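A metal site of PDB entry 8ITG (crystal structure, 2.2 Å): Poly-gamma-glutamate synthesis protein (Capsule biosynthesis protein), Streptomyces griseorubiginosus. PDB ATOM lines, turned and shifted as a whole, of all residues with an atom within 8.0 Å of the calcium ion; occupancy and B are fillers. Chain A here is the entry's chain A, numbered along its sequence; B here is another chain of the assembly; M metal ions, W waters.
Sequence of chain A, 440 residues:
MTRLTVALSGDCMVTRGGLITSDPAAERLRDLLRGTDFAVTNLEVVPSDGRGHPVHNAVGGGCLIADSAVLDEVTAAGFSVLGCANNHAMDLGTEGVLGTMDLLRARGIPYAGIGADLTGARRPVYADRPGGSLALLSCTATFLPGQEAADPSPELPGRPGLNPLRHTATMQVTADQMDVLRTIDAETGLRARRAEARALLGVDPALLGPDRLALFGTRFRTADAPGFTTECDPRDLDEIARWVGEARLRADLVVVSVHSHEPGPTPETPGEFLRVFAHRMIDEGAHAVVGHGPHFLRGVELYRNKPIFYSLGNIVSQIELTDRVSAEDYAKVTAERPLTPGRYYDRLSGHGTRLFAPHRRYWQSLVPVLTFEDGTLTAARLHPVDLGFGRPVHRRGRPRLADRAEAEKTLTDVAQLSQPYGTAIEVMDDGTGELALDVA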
ATOM      1  N   ASP A  11       4.774 -13.613  -1.355  1.00  0.00           N
ATOM      2  CA  ASP A  11       4.697 -12.382  -0.592  1.00  0.00           C
ATOM      3  C   ASP A  11       3.338 -11.707  -0.766  1.00  0.00           C
ATOM      4  O   ASP A  11       2.905 -11.445  -1.896  1.00  0.00           O
ATOM      5  CB  ASP A  11       5.810 -11.426  -1.018  1.00  0.00           C
ATOM      6  CG  ASP A  11       7.184 -11.930  -0.646  1.00  0.00           C
ATOM      7  OD1 ASP A  11       7.269 -12.812   0.240  1.00  0.00           O
ATOM      8  OD2 ASP A  11       8.177 -11.436  -1.224  1.00  0.00           O
ATOM      9  N   MET A  13       2.051  -8.396  -0.126  1.00  0.00           N
ATOM     10  CA  MET A  13       2.340  -6.993   0.168  1.00  0.00           C
ATOM     11  C   MET A  13       1.096  -6.174  -0.138  1.00  0.00           C
ATOM     12  O   MET A  13       1.009  -5.459  -1.144  1.00  0.00           O
ATOM     13  CB  MET A  13       3.547  -6.514  -0.637  1.00  0.00           C
ATOM     14  CG  MET A  13       4.780  -7.370  -0.494  1.00  0.00           C
ATOM     15  SD  MET A  13       6.221  -6.737  -1.391  1.00  0.00           S
ATOM     16  CE  MET A  13       5.730  -7.047  -3.078  1.00  0.00           C
ATOM     17  N   ASN A  42       2.661 -15.262   3.023  1.00  0.00           N
ATOM     18  CA  ASN A  42       3.667 -14.550   3.787  1.00  0.00           C
ATOM     19  C   ASN A  42       3.222 -13.097   3.924  1.00  0.00           C
ATOM     20  O   ASN A  42       3.215 -12.353   2.946  1.00  0.00           O
ATOM     21  CB  ASN A  42       5.041 -14.636   3.122  1.00  0.00           C
ATOM     22  CG  ASN A  42       6.050 -13.691   3.744  1.00  0.00           C
ATOM     23  OD1 ASN A  42       6.326 -13.763   4.939  1.00  0.00           O
ATOM     24  ND2 ASN A  42       6.608 -12.799   2.931  1.00  0.00           N
ATOM     25  N   GLU A  44       3.796  -9.827   4.115  1.00  0.00           N
ATOM     26  CA  GLU A  44       4.938  -8.951   3.829  1.00  0.00           C
ATOM     27  C   GLU A  44       4.539  -7.485   3.976  1.00  0.00           C
ATOM     28  O   GLU A  44       4.688  -6.672   3.068  1.00  0.00           O
ATOM     29  CB  GLU A  44       5.486  -9.251   2.441  1.00  0.00           C
ATOM     30  CG  GLU A  44       6.783  -8.552   2.069  1.00  0.00           C
ATOM     31  CD  GLU A  44       8.004  -9.262   2.589  1.00  0.00           C
ATOM     32  OE1 GLU A  44       7.842 -10.295   3.257  1.00  0.00           O
ATOM     33  OE2 GLU A  44       9.122  -8.789   2.312  1.00  0.00           O
ATOM     34  N   ASN A  57      14.979   0.992   6.992  1.00  0.00           N
ATOM     35  CA  ASN A  57      15.034  -0.229   6.197  1.00  0.00           C
ATOM     36  C   ASN A  57      15.242   0.105   4.728  1.00  0.00           C
ATOM     37  O   ASN A  57      14.484  -0.332   3.863  1.00  0.00           O
ATOM     38  CB  ASN A  57      13.766  -1.049   6.403  1.00  0.00           C
ATOM     39  CG  ASN A  57      13.896  -2.470   5.884  1.00  0.00           C
ATOM     40  OD1 ASN A  57      14.986  -2.909   5.515  1.00  0.00           O
ATOM     41  ND2 ASN A  57      12.781  -3.198   5.855  1.00  0.00           N
ATOM     42  N   GLY A  60      15.837  -2.973   2.599  1.00  0.00           N
ATOM     43  CA  GLY A  60      14.600  -3.650   2.277  1.00  0.00           C
ATOM     44  C   GLY A  60      13.684  -2.920   1.314  1.00  0.00           C
ATOM     45  O   GLY A  60      12.591  -3.416   1.021  1.00  0.00           O
ATOM     46  N   LEU A  64       7.165  -0.803   4.949  1.00  0.00           N
ATOM     47  CA  LEU A  64       5.984  -1.433   4.358  1.00  0.00           C
ATOM     48  C   LEU A  64       4.939  -1.534   5.460  1.00  0.00           C
ATOM     49  O   LEU A  64       4.877  -2.535   6.182  1.00  0.00           O
ATOM     50  CB  LEU A  64       6.343  -2.787   3.753  1.00  0.00           C
ATOM     51  CG  LEU A  64       5.497  -3.347   2.612  1.00  0.00           C
ATOM     52  CD1 LEU A  64       4.951  -2.223   1.749  1.00  0.00           C
ATOM     53  CD2 LEU A  64       6.344  -4.291   1.776  1.00  0.00           C
ATOM     54  N   ALA A  85       7.550 -14.184   9.403  1.00  0.00           N
ATOM     55  CA  ALA A  85       8.980 -13.932   9.465  1.00  0.00           C
ATOM     56  C   ALA A  85       9.482 -13.488   8.096  1.00  0.00           C
ATOM     57  O   ALA A  85       9.453 -14.269   7.131  1.00  0.00           O
ATOM     58  CB  ALA A  85       9.737 -15.156   9.951  1.00  0.00           C
ATOM     59  N   ASN A  86       9.942 -12.249   8.004  1.00  0.00           N
ATOM     60  CA  ASN A  86      10.457 -11.669   6.769  1.00  0.00           C
ATOM     61  C   ASN A  86      11.174 -10.370   7.121  1.00  0.00           C
ATOM     62  O   ASN A  86      11.173  -9.946   8.279  1.00  0.00           O
ATOM     63  CB  ASN A  86       9.342 -11.441   5.740  1.00  0.00           C
ATOM     64  CG  ASN A  86       8.201 -10.604   6.291  1.00  0.00           C
ATOM     65  OD1 ASN A  86       8.421  -9.518   6.847  1.00  0.00           O
ATOM     66  ND2 ASN A  86       6.981 -11.093   6.152  1.00  0.00           N
ATOM     67  N   ASN A  87      11.775  -9.734   6.119  1.00  0.00           N
ATOM     68  CA  ASN A  87      12.562  -8.524   6.351  1.00  0.00           C
ATOM     69  C   ASN A  87      11.697  -7.281   6.528  1.00  0.00           C
ATOM     70  O   ASN A  87      12.250  -6.166   6.519  1.00  0.00           O
ATOM     71  CB  ASN A  87      13.545  -8.298   5.198  1.00  0.00           C
ATOM     72  CG  ASN A  87      12.842  -8.130   3.874  1.00  0.00           C
ATOM     73  OD1 ASN A  87      11.943  -8.893   3.554  1.00  0.00           O
ATOM     74  ND2 ASN A  87      13.242  -7.115   3.112  1.00  0.00           N
ATOM     75  N   HIS A  88      10.385  -7.419   6.690  1.00  0.00           N
ATOM     76  CA  HIS A  88       9.527  -6.253   6.902  1.00  0.00           C
ATOM     77  C   HIS A  88       8.674  -6.328   8.148  1.00  0.00           C
ATOM     78  O   HIS A  88       8.108  -5.305   8.538  1.00  0.00           O
ATOM     79  CB  HIS A  88       8.610  -6.031   5.683  1.00  0.00           C
ATOM     80  CG  HIS A  88       9.310  -5.360   4.537  1.00  0.00           C
ATOM     81  ND1 HIS A  88       9.644  -4.014   4.557  1.00  0.00           N
ATOM     82  CD2 HIS A  88       9.754  -5.840   3.357  1.00  0.00           C
ATOM     83  CE1 HIS A  88      10.258  -3.708   3.433  1.00  0.00           C
ATOM     84  NE2 HIS A  88      10.335  -4.791   2.685  1.00  0.00           N
ATOM     85  N   ALA A  89       8.556  -7.495   8.797  1.00  0.00           N
ATOM     86  CA  ALA A  89       7.739  -7.602  10.005  1.00  0.00           C
ATOM     87  C   ALA A  89       8.186  -6.626  11.079  1.00  0.00           C
ATOM     88  O   ALA A  89       7.369  -6.196  11.911  1.00  0.00           O
ATOM     89  CB  ALA A  89       7.790  -9.038  10.531  1.00  0.00           C
ATOM     90  N   THR A 140      13.012 -16.487   8.455  1.00  0.00           N
ATOM     91  CA  THR A 140      13.527 -15.638   7.391  1.00  0.00           C
ATOM     92  C   THR A 140      15.046 -15.588   7.445  1.00  0.00           C
ATOM     93  O   THR A 140      15.639 -15.442   8.517  1.00  0.00           O
ATOM     94  CB  THR A 140      12.958 -14.213   7.477  1.00  0.00           C
ATOM     95  OG1 THR A 140      13.565 -13.395   6.475  1.00  0.00           O
ATOM     96  CG2 THR A 140      13.202 -13.584   8.846  1.00  0.00           C
ATOM     97  N   THR A 142      16.519 -13.239   5.545  1.00  0.00           N
ATOM     98  CA  THR A 142      16.762 -11.857   5.147  1.00  0.00           C
ATOM     99  C   THR A 142      16.146 -10.953   6.202  1.00  0.00           C
ATOM    100  O   THR A 142      14.924 -10.944   6.390  1.00  0.00           O
ATOM    101  CB  THR A 142      16.172 -11.567   3.769  1.00  0.00           C
ATOM    102  OG1 THR A 142      16.649 -12.539   2.827  1.00  0.00           O
ATOM    103  CG2 THR A 142      16.564 -10.166   3.300  1.00  0.00           C
ATOM    104  N   HIS A 259      11.575 -17.095   4.245  1.00  0.00           N
ATOM    105  CA  HIS A 259      11.814 -15.898   3.450  1.00  0.00           C
ATOM    106  C   HIS A 259      13.305 -15.802   3.143  1.00  0.00           C
ATOM    107  O   HIS A 259      14.129 -15.892   4.059  1.00  0.00           O
ATOM    108  CB  HIS A 259      11.340 -14.664   4.215  1.00  0.00           C
ATOM    109  CG  HIS A 259      11.071 -13.476   3.347  1.00  0.00           C
ATOM    110  ND1 HIS A 259      10.020 -13.419   2.461  1.00  0.00           N
ATOM    111  CD2 HIS A 259      11.701 -12.285   3.260  1.00  0.00           C
ATOM    112  CE1 HIS A 259      10.024 -12.250   1.851  1.00  0.00           C
ATOM    113  NE2 HIS A 259      11.036 -11.533   2.316  1.00  0.00           N
ATOM    114  N   SER A 260      13.645 -15.623   1.868  1.00  0.00           N
ATOM    115  CA  SER A 260      15.055 -15.605   1.477  1.00  0.00           C
ATOM    116  C   SER A 260      15.211 -14.807   0.191  1.00  0.00           C
ATOM    117  O   SER A 260      14.774 -15.259  -0.876  1.00  0.00           O
ATOM    118  CB  SER A 260      15.580 -17.023   1.303  1.00  0.00           C
ATOM    119  OG  SER A 260      16.968 -17.022   1.021  1.00  0.00           O
ATOM    120  N   HIS A 261      15.842 -13.631   0.282  1.00  0.00           N
ATOM    121  CA  HIS A 261      16.211 -12.865  -0.896  1.00  0.00           C
ATOM    122  C   HIS A 261      17.536 -13.312  -1.500  1.00  0.00           C
ATOM    123  O   HIS A 261      17.830 -12.943  -2.643  1.00  0.00           O
ATOM    124  CB  HIS A 261      16.328 -11.377  -0.572  1.00  0.00           C
ATOM    125  CG  HIS A 261      15.023 -10.710  -0.254  1.00  0.00           C
ATOM    126  ND1 HIS A 261      14.456  -9.770  -1.086  1.00  0.00           N
ATOM    127  CD2 HIS A 261      14.193 -10.828   0.806  1.00  0.00           C
ATOM    128  CE1 HIS A 261      13.325  -9.343  -0.550  1.00  0.00           C
ATOM    129  NE2 HIS A 261      13.139  -9.966   0.589  1.00  0.00           N
ATOM    130  N   HIS A 292       9.917 -17.626  -0.512  1.00  0.00           N
ATOM    131  CA  HIS A 292       9.499 -16.334  -1.031  1.00  0.00           C
ATOM    132  C   HIS A 292      10.604 -15.344  -0.695  1.00  0.00           C
ATOM    133  O   HIS A 292      11.561 -15.674   0.001  1.00  0.00           O
ATOM    134  CB  HIS A 292       8.144 -15.911  -0.460  1.00  0.00           C
ATOM    135  CG  HIS A 292       7.907 -16.399   0.933  1.00  0.00           C
ATOM    136  ND1 HIS A 292       8.566 -15.883   2.028  1.00  0.00           N
ATOM    137  CD2 HIS A 292       7.094 -17.384   1.400  1.00  0.00           C
ATOM    138  CE1 HIS A 292       8.161 -16.525   3.118  1.00  0.00           C
ATOM    139  NE2 HIS A 292       7.278 -17.433   2.768  1.00  0.00           N
ATOM    140  N   GLY A 293      10.471 -14.119  -1.206  1.00  0.00           N
ATOM    141  CA  GLY A 293      11.488 -13.114  -1.033  1.00  0.00           C
ATOM    142  C   GLY A 293      11.869 -12.370  -2.297  1.00  0.00           C
ATOM    143  O   GLY A 293      11.743 -11.150  -2.369  1.00  0.00           O
ATOM    144  N   PRO A 294      12.348 -13.090  -3.317  1.00  0.00           N
ATOM    145  CA  PRO A 294      12.927 -12.417  -4.494  1.00  0.00           C
ATOM    146  C   PRO A 294      11.944 -11.612  -5.329  1.00  0.00           C
ATOM    147  O   PRO A 294      12.403 -10.859  -6.196  1.00  0.00           O
ATOM    148  CB  PRO A 294      13.515 -13.571  -5.313  1.00  0.00           C
ATOM    149  CG  PRO A 294      13.692 -14.690  -4.337  1.00  0.00           C
ATOM    150  CD  PRO A 294      12.550 -14.553  -3.382  1.00  0.00           C
ATOM    151  N   HIS A 295      10.637 -11.762  -5.133  1.00  0.00           N
ATOM    152  CA  HIS A 295       9.565 -11.124  -5.903  1.00  0.00           C
ATOM    153  C   HIS A 295       9.438 -11.697  -7.312  1.00  0.00           C
ATOM    154  O   HIS A 295       8.641 -11.173  -8.109  1.00  0.00           O
ATOM    155  CB  HIS A 295       9.724  -9.601  -6.008  1.00  0.00           C
ATOM    156  CG  HIS A 295       9.878  -8.929  -4.679  1.00  0.00           C
ATOM    157  ND1 HIS A 295       8.905  -8.994  -3.698  1.00  0.00           N
ATOM    158  CD2 HIS A 295      10.877  -8.173  -4.171  1.00  0.00           C
ATOM    159  CE1 HIS A 295       9.304  -8.304  -2.649  1.00  0.00           C
ATOM    160  NE2 HIS A 295      10.495  -7.794  -2.897  1.00  0.00           N
ATOM    161  N   ASN A 314       5.444 -12.876  -5.531  1.00  0.00           N
ATOM    162  CA  ASN A 314       4.447 -12.068  -4.859  1.00  0.00           C
ATOM    163  C   ASN A 314       3.058 -12.571  -5.202  1.00  0.00           C
ATOM    164  O   ASN A 314       2.766 -12.855  -6.368  1.00  0.00           O
ATOM    165  CB  ASN A 314       4.555 -10.592  -5.265  1.00  0.00           C
ATOM    166  CG  ASN A 314       5.967 -10.063  -5.144  1.00  0.00           C
ATOM    167  OD1 ASN A 314       6.681 -10.365  -4.190  1.00  0.00           O
ATOM    168  ND2 ASN A 314       6.374  -9.266  -6.119  1.00  0.00           N
ATOM    169  N   ILE A 319       3.442  -2.226  -3.142  1.00  0.00           N
ATOM    170  CA  ILE A 319       4.446  -1.385  -2.470  1.00  0.00           C
ATOM    171  C   ILE A 319       4.233   0.078  -2.824  1.00  0.00           C
ATOM    172  O   ILE A 319       4.182   0.957  -1.951  1.00  0.00           O
ATOM    173  CB  ILE A 319       5.871  -1.844  -2.849  1.00  0.00           C
ATOM    174  CG1 ILE A 319       6.116  -3.295  -2.456  1.00  0.00           C
ATOM    175  CG2 ILE A 319       6.910  -0.928  -2.202  1.00  0.00           C
ATOM    176  CD1 ILE A 319       7.479  -3.806  -2.879  1.00  0.00           C
ATOM    177  N   CYS B  40      18.305  -6.192  -1.457  1.00  0.00           N
ATOM    178  CA  CYS B  40      17.194  -7.112  -1.274  1.00  0.00           C
ATOM    179  C   CYS B  40      15.893  -6.340  -1.020  1.00  0.00           C
ATOM    180  O   CYS B  40      15.508  -6.087   0.119  1.00  0.00           O
ATOM    181  CB  CYS B  40      17.493  -8.094  -0.125  1.00  0.00           C
ATOM    182  SG  CYS B  40      18.288  -7.422   1.377  1.00  0.00           S
ATOM    183  N   PHE B  41      15.233  -5.976  -2.114  1.00  0.00           N
ATOM    184  CA  PHE B  41      14.156  -4.992  -2.108  1.00  0.00           C
ATOM    185  C   PHE B  41      12.832  -5.624  -1.698  1.00  0.00           C
ATOM    186  O   PHE B  41      12.585  -6.804  -1.932  1.00  0.00           O
ATOM    187  CB  PHE B  41      14.032  -4.371  -3.502  1.00  0.00           C
ATOM    188  CG  PHE B  41      13.717  -2.897  -3.498  1.00  0.00           C
ATOM    189  CD1 PHE B  41      14.718  -1.966  -3.713  1.00  0.00           C
ATOM    190  CD2 PHE B  41      12.413  -2.445  -3.329  1.00  0.00           C
ATOM    191  CE1 PHE B  41      14.434  -0.610  -3.727  1.00  0.00           C
ATOM    192  CE2 PHE B  41      12.123  -1.082  -3.342  1.00  0.00           C
ATOM    193  CZ  PHE B  41      13.139  -0.166  -3.545  1.00  0.00           C
ATOM    194  N   GLY B  42      11.975  -4.806  -1.081  1.00  0.00           N
ATOM    195  CA  GLY B  42      10.588  -5.168  -0.842  1.00  0.00           C
ATOM    196  C   GLY B  42      10.346  -6.375   0.039  1.00  0.00           C
ATOM    197  O   GLY B  42      11.284  -6.928   0.623  1.00  0.00           O
ATOM    198  OXT GLY B  42       9.213  -6.823   0.190  1.00  0.00           O
HETATM  199 CA    CA M   1      11.097  -9.329   1.468  1.00  0.00          CA
HETATM  200  O   HOH W   1      10.155 -10.066  -0.481  1.00  0.00           O
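The side-chain amide nitrogen (ND2) of Asn 42 of chain A is in hydrogen-bond range of the side-chain carboxylate (OE1) of Glu 44. A ring nitrogen (ND1) of His 259 lies within hydrogen-bond range of the side-chain amide nitrogen of Asn 42 of chain A, 3.5 Å away. The backbone carbonyl oxygen of Gly 293 lies close to a ring nitrogen (ND1) of His 261, at 3.3 Å. NE2 of His 295 sits close to OXT of Gly 42 of chain B (3.5 Å). ND1 of His 292 is in hydrogen-bond range of ND1 of His 259, 2.9 Å away. The chain-end carboxylate of Gly 42 of chain B lies close to a ring nitrogen (NE2) of His 88 (3.4 Å). O of Asn 87 lies within hydrogen-bond range of ND2 of Asn 57, at 3.1 Å. N of Asn 87 lies close to O of Thr 142, 3.4 Å away.
Of the 26 residues printed, 5 come within 4 Å of the calcium ion. The nearest printed residue that does not touch the calcium ion is His 88 (4.2 Å).
The calcium ion is bound by OE2 of Glu 44 (2.2 Å), water W1 (2.3 Å), OD1 of Asn 87 (2.3 Å), NE2 of His 261 (2.3 Å), NE2 of His 259 (2.4 Å) and O of Gly 42 of chain B (2.6 Å). The calcium ion has six donor atoms within binding distance.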
